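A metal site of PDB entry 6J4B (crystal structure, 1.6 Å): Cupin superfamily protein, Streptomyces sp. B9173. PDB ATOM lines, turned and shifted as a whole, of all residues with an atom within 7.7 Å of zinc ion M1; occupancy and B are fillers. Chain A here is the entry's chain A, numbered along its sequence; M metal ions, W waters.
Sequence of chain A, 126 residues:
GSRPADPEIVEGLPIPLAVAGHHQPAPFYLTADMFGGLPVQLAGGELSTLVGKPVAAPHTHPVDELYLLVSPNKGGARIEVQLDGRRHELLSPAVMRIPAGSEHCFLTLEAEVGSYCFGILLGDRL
O of Glu 65 sits at hydrogen-bond distance from N of Ile 98, at 2.8 Å.
ND1 of His 104 sits at hydrogen-bond distance from O of Ser 102 (2.9 Å).
N of His 104 is in hydrogen-bond range of O of His 59, at 2.9 Å.
Merely in contact with zinc ion M1: Tyr 67 (3.8 Å).
Within 4 Å of zinc ion M1: His 61, Glu 65, Tyr 67 and His 104.
The nearest printed residue that does not touch zinc ion M1 is His 59 (4.03 Å).
OE1 of Glu 65 binds zinc ion M1.
Zinc ion M1 is bound by water W1 (2.0 Å).
NE2 of His 61 binds zinc ion M1, 2.0 Å away.
NE2 of His 104 is bound to zinc ion M1, at 2.1 Å.
Slightly farther from zinc ion M1 lies the side-chain carboxylate (OE2) of Glu 65 (2.8 Å).
Water W1 bridges OH of Tyr 67 and OE2 of Glu 65.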
ATOM      1  N   VAL A  19      -7.298  -2.931  16.355  1.00  0.00           N
ATOM      2  CA  VAL A  19      -7.460  -4.386  16.233  1.00  0.00           C
ATOM      3  C   VAL A  19      -8.772  -4.691  15.482  1.00  0.00           C
ATOM      4  O   VAL A  19      -9.798  -4.063  15.772  1.00  0.00           O
ATOM      5  CB  VAL A  19      -7.511  -5.070  17.643  1.00  0.00           C
ATOM      6  CG1 VAL A  19      -7.739  -6.547  17.557  1.00  0.00           C
ATOM      7  CG2 VAL A  19      -6.175  -4.825  18.387  1.00  0.00           C
ATOM      8  N   HIS A  22     -12.837  -4.371  16.492  1.00  0.00           N
ATOM      9  CA  HIS A  22     -13.059  -3.369  17.530  1.00  0.00           C
ATOM     10  C   HIS A  22     -13.530  -2.047  16.986  1.00  0.00           C
ATOM     11  O   HIS A  22     -13.446  -1.827  15.769  1.00  0.00           O
ATOM     12  CB  HIS A  22     -11.722  -3.175  18.324  1.00  0.00           C
ATOM     13  CG  HIS A  22     -11.290  -4.404  19.109  1.00  0.00           C
ATOM     14  ND1 HIS A  22     -11.007  -5.616  18.544  1.00  0.00           N
ATOM     15  CD2 HIS A  22     -11.122  -4.554  20.437  1.00  0.00           C
ATOM     16  CE1 HIS A  22     -10.627  -6.466  19.484  1.00  0.00           C
ATOM     17  NE2 HIS A  22     -10.685  -5.826  20.642  1.00  0.00           N
ATOM     18  N   HIS A  59     -13.464 -11.801  16.157  1.00  0.00           N
ATOM     19  CA  HIS A  59     -12.203 -11.553  15.537  1.00  0.00           C
ATOM     20  C   HIS A  59     -11.280 -12.710  15.829  1.00  0.00           C
ATOM     21  O   HIS A  59     -11.607 -13.607  16.598  1.00  0.00           O
ATOM     22  CB  HIS A  59     -11.609 -10.190  15.995  1.00  0.00           C
ATOM     23  CG  HIS A  59     -11.490 -10.061  17.507  1.00  0.00           C
ATOM     24  ND1 HIS A  59     -12.612  -9.866  18.273  1.00  0.00           N
ATOM     25  CD2 HIS A  59     -10.449 -10.149  18.361  1.00  0.00           C
ATOM     26  CE1 HIS A  59     -12.276  -9.849  19.557  1.00  0.00           C
ATOM     27  NE2 HIS A  59     -10.962 -10.001  19.623  1.00  0.00           N
ATOM     28  N   THR A  60     -10.188 -12.723  15.077  1.00  0.00           N
ATOM     29  CA  THR A  60      -9.150 -13.804  15.177  1.00  0.00           C
ATOM     30  C   THR A  60      -7.741 -13.262  15.390  1.00  0.00           C
ATOM     31  O   THR A  60      -7.484 -12.119  15.088  1.00  0.00           O
ATOM     32  CB  THR A  60      -9.108 -14.694  13.892  1.00  0.00           C
ATOM     33  OG1 THR A  60      -8.594 -13.916  12.783  1.00  0.00           O
ATOM     34  CG2 THR A  60     -10.481 -15.265  13.531  1.00  0.00           C
ATOM     35  N   HIS A  61      -6.853 -14.108  15.936  1.00  0.00           N
ATOM     36  CA  HIS A  61      -5.438 -13.883  15.937  1.00  0.00           C
ATOM     37  C   HIS A  61      -4.751 -15.122  15.256  1.00  0.00           C
ATOM     38  O   HIS A  61      -5.273 -16.236  15.306  1.00  0.00           O
ATOM     39  CB  HIS A  61      -4.893 -13.790  17.375  1.00  0.00           C
ATOM     40  CG  HIS A  61      -5.774 -13.006  18.321  1.00  0.00           C
ATOM     41  ND1 HIS A  61      -5.992 -11.650  18.192  1.00  0.00           N
ATOM     42  CD2 HIS A  61      -6.505 -13.406  19.382  1.00  0.00           C
ATOM     43  CE1 HIS A  61      -6.807 -11.257  19.181  1.00  0.00           C
ATOM     44  NE2 HIS A  61      -7.139 -12.321  19.901  1.00  0.00           N
ATOM     45  N   VAL A  63      -2.168 -16.521  16.482  1.00  0.00           N
ATOM     46  CA  VAL A  63      -1.532 -17.270  17.561  1.00  0.00           C
ATOM     47  C   VAL A  63      -2.564 -17.656  18.589  1.00  0.00           C
ATOM     48  O   VAL A  63      -3.609 -17.003  18.653  1.00  0.00           O
ATOM     49  CB  VAL A  63      -0.360 -16.475  18.199  1.00  0.00           C
ATOM     50  CG1 VAL A  63       0.683 -16.094  17.121  1.00  0.00           C
ATOM     51  CG2 VAL A  63      -0.855 -15.179  18.822  1.00  0.00           C
ATOM     52  N   ASP A  64      -2.304 -18.706  19.389  1.00  0.00           N
ATOM     53  CA  ASP A  64      -3.151 -19.044  20.507  1.00  0.00           C
ATOM     54  C   ASP A  64      -3.158 -17.857  21.522  1.00  0.00           C
ATOM     55  O   ASP A  64      -2.187 -17.100  21.632  1.00  0.00           O
ATOM     56  CB  ASP A  64      -2.695 -20.290  21.256  1.00  0.00           C
ATOM     57  CG  ASP A  64      -2.847 -21.540  20.483  1.00  0.00           C
ATOM     58  OD1 ASP A  64      -3.586 -21.574  19.457  1.00  0.00           O
ATOM     59  OD2 ASP A  64      -2.195 -22.526  20.933  1.00  0.00           O
ATOM     60  N   GLU A  65      -4.228 -17.803  22.281  1.00  0.00           N
ATOM     61  CA  GLU A  65      -4.385 -16.678  23.297  1.00  0.00           C
ATOM     62  C   GLU A  65      -5.015 -17.345  24.514  1.00  0.00           C
ATOM     63  O   GLU A  65      -5.799 -18.300  24.410  1.00  0.00           O
ATOM     64  CB  GLU A  65      -5.321 -15.611  22.822  1.00  0.00           C
ATOM     65  CG  GLU A  65      -5.631 -14.447  23.755  1.00  0.00           C
ATOM     66  CD  GLU A  65      -6.559 -13.516  23.102  1.00  0.00           C
ATOM     67  OE1 GLU A  65      -7.565 -13.949  22.469  1.00  0.00           O
ATOM     68  OE2 GLU A  65      -6.337 -12.337  23.239  1.00  0.00           O
ATOM     69  N   LEU A  66      -4.656 -16.837  25.676  1.00  0.00           N
ATOM     70  CA  LEU A  66      -5.249 -17.250  26.920  1.00  0.00           C
ATOM     71  C   LEU A  66      -5.962 -16.081  27.609  1.00  0.00           C
ATOM     72  O   LEU A  66      -5.336 -15.009  27.791  1.00  0.00           O
ATOM     73  CB  LEU A  66      -4.206 -17.808  27.924  1.00  0.00           C
ATOM     74  CG  LEU A  66      -3.270 -18.869  27.346  1.00  0.00           C
ATOM     75  CD1 LEU A  66      -2.159 -19.319  28.242  1.00  0.00           C
ATOM     76  CD2 LEU A  66      -4.097 -20.059  26.896  1.00  0.00           C
ATOM     77  N   TYR A  67      -7.245 -16.241  27.882  1.00  0.00           N
ATOM     78  CA  TYR A  67      -8.003 -15.235  28.663  1.00  0.00           C
ATOM     79  C   TYR A  67      -7.782 -15.525  30.126  1.00  0.00           C
ATOM     80  O   TYR A  67      -7.882 -16.677  30.554  1.00  0.00           O
ATOM     81  CB  TYR A  67      -9.491 -15.281  28.316  1.00  0.00           C
ATOM     82  CG  TYR A  67      -9.932 -14.489  27.165  1.00  0.00           C
ATOM     83  CD1 TYR A  67      -9.052 -14.013  26.244  1.00  0.00           C
ATOM     84  CD2 TYR A  67     -11.234 -14.356  26.893  1.00  0.00           C
ATOM     85  CE1 TYR A  67      -9.490 -13.191  25.163  1.00  0.00           C
ATOM     86  CE2 TYR A  67     -11.694 -13.568  25.827  1.00  0.00           C
ATOM     87  CZ  TYR A  67     -10.809 -12.975  24.990  1.00  0.00           C
ATOM     88  OH  TYR A  67     -11.313 -12.175  23.932  1.00  0.00           O
ATOM     89  N   ILE A  98      -8.069 -19.779  23.847  1.00  0.00           N
ATOM     90  CA  ILE A  98      -8.645 -19.306  22.585  1.00  0.00           C
ATOM     91  C   ILE A  98      -7.696 -19.757  21.453  1.00  0.00           C
ATOM     92  O   ILE A  98      -6.637 -19.183  21.223  1.00  0.00           O
ATOM     93  CB  ILE A  98      -8.768 -17.776  22.574  1.00  0.00           C
ATOM     94  CG1 ILE A  98      -9.450 -17.187  23.837  1.00  0.00           C
ATOM     95  CG2 ILE A  98      -9.483 -17.327  21.278  1.00  0.00           C
ATOM     96  CD1 ILE A  98     -10.857 -17.671  24.006  1.00  0.00           C
ATOM     97  N   SER A 102      -9.513 -19.091  15.810  1.00  0.00           N
ATOM     98  CA  SER A 102     -10.821 -19.176  16.303  1.00  0.00           C
ATOM     99  C   SER A 102     -11.470 -17.813  16.290  1.00  0.00           C
ATOM    100  O   SER A 102     -10.847 -16.813  16.784  1.00  0.00           O
ATOM    101  CB  SER A 102     -10.828 -19.690  17.725  1.00  0.00           C
ATOM    102  OG  SER A 102     -12.133 -19.696  18.239  1.00  0.00           O
ATOM    103  N   HIS A 104     -13.715 -15.186  17.865  1.00  0.00           N
ATOM    104  CA  HIS A 104     -14.084 -15.078  19.254  1.00  0.00           C
ATOM    105  C   HIS A 104     -14.235 -13.634  19.662  1.00  0.00           C
ATOM    106  O   HIS A 104     -13.837 -12.685  18.956  1.00  0.00           O
ATOM    107  CB  HIS A 104     -13.020 -15.733  20.173  1.00  0.00           C
ATOM    108  CG  HIS A 104     -11.707 -15.002  20.124  1.00  0.00           C
ATOM    109  ND1 HIS A 104     -10.805 -15.094  19.084  1.00  0.00           N
ATOM    110  CD2 HIS A 104     -11.184 -14.089  20.980  1.00  0.00           C
ATOM    111  CE1 HIS A 104      -9.765 -14.321  19.335  1.00  0.00           C
ATOM    112  NE2 HIS A 104     -10.009 -13.678  20.467  1.00  0.00           N
ATOM    113  N   CYS A 105     -14.890 -13.495  20.820  1.00  0.00           N
ATOM    114  CA  CYS A 105     -15.134 -12.180  21.433  1.00  0.00           C
ATOM    115  C   CYS A 105     -15.703 -12.420  22.811  1.00  0.00           C
ATOM    116  O   CYS A 105     -16.096 -13.550  23.100  1.00  0.00           O
ATOM    117  CB  CYS A 105     -16.029 -11.314  20.611  1.00  0.00           C
ATOM    118  SG  CYS A 105     -17.570 -12.052  20.181  1.00  0.00           S
ATOM    119  N   PHE A 106     -15.753 -11.373  23.600  1.00  0.00           N
ATOM    120  CA  PHE A 106     -16.312 -11.517  24.970  1.00  0.00           C
ATOM    121  C   PHE A 106     -17.303 -10.403  25.287  1.00  0.00           C
ATOM    122  O   PHE A 106     -17.258  -9.286  24.711  1.00  0.00           O
ATOM    123  CB  PHE A 106     -15.278 -11.658  26.100  1.00  0.00           C
ATOM    124  CG  PHE A 106     -14.699 -10.363  26.594  1.00  0.00           C
ATOM    125  CD1 PHE A 106     -13.653  -9.699  25.918  1.00  0.00           C
ATOM    126  CD2 PHE A 106     -15.125  -9.776  27.770  1.00  0.00           C
ATOM    127  CE1 PHE A 106     -13.182  -8.472  26.385  1.00  0.00           C
ATOM    128  CE2 PHE A 106     -14.627  -8.623  28.257  1.00  0.00           C
ATOM    129  CZ  PHE A 106     -13.630  -7.925  27.582  1.00  0.00           C
ATOM    130  N   GLY A 119      -5.992 -10.737  27.799  1.00  0.00           N
ATOM    131  CA  GLY A 119      -5.694 -11.758  26.810  1.00  0.00           C
ATOM    132  C   GLY A 119      -4.214 -11.837  26.585  1.00  0.00           C
ATOM    133  O   GLY A 119      -3.548 -10.785  26.272  1.00  0.00           O
ATOM    134  N   ILE A 120      -3.624 -12.967  26.908  1.00  0.00           N
ATOM    135  CA  ILE A 120      -2.202 -13.247  26.741  1.00  0.00           C
ATOM    136  C   ILE A 120      -2.017 -13.953  25.419  1.00  0.00           C
ATOM    137  O   ILE A 120      -2.413 -15.090  25.263  1.00  0.00           O
ATOM    138  CB  ILE A 120      -1.590 -14.023  27.926  1.00  0.00           C
ATOM    139  CG1 ILE A 120      -1.754 -13.312  29.333  1.00  0.00           C
ATOM    140  CG2 ILE A 120      -0.137 -14.304  27.667  1.00  0.00           C
ATOM    141  CD1 ILE A 120      -3.018 -13.634  30.080  1.00  0.00           C
ATOM    142  N   LEU A 121      -1.405 -13.239  24.464  1.00  0.00           N
ATOM    143  CA  LEU A 121      -1.207 -13.732  23.092  1.00  0.00           C
ATOM    144  C   LEU A 121       0.153 -14.468  23.019  1.00  0.00           C
ATOM    145  O   LEU A 121       1.221 -13.863  23.326  1.00  0.00           O
ATOM    146  CB  LEU A 121      -1.230 -12.602  22.092  1.00  0.00           C
ATOM    147  CG  LEU A 121      -2.558 -11.881  21.974  1.00  0.00           C
ATOM    148  CD1 LEU A 121      -2.347 -10.386  21.700  1.00  0.00           C
ATOM    149  CD2 LEU A 121      -3.457 -12.580  20.973  1.00  0.00           C
ATOM    150  N   LEU A 126      -0.151 -10.110  15.486  1.00  0.00           N
ATOM    151  CA  LEU A 126      -1.582  -9.984  15.505  1.00  0.00           C
ATOM    152  C   LEU A 126      -2.195 -10.323  14.153  1.00  0.00           C
ATOM    153  O   LEU A 126      -3.418 -10.397  14.114  1.00  0.00           O
ATOM    154  CB  LEU A 126      -1.990  -8.538  15.844  1.00  0.00           C
ATOM    155  CG  LEU A 126      -1.715  -8.100  17.283  1.00  0.00           C
ATOM    156  CD1 LEU A 126      -1.995  -6.590  17.429  1.00  0.00           C
ATOM    157  CD2 LEU A 126      -2.584  -8.950  18.190  1.00  0.00           C
ATOM    158  OXT LEU A 126      -1.457 -10.465  13.129  1.00  0.00           O
HETATM  159 ZN    ZN M   1      -8.474 -12.615  21.426  1.00  0.00          ZN
HETATM  160 ZN    ZN M   2      -9.968  -9.650  21.353  1.00  0.00          ZN
HETATM  161 ZN    ZN M   3     -10.109  -6.646  22.414  1.00  0.00          ZN
HETATM  162  O   HOH W   1      -9.371 -11.154  22.385  1.00  0.00           O
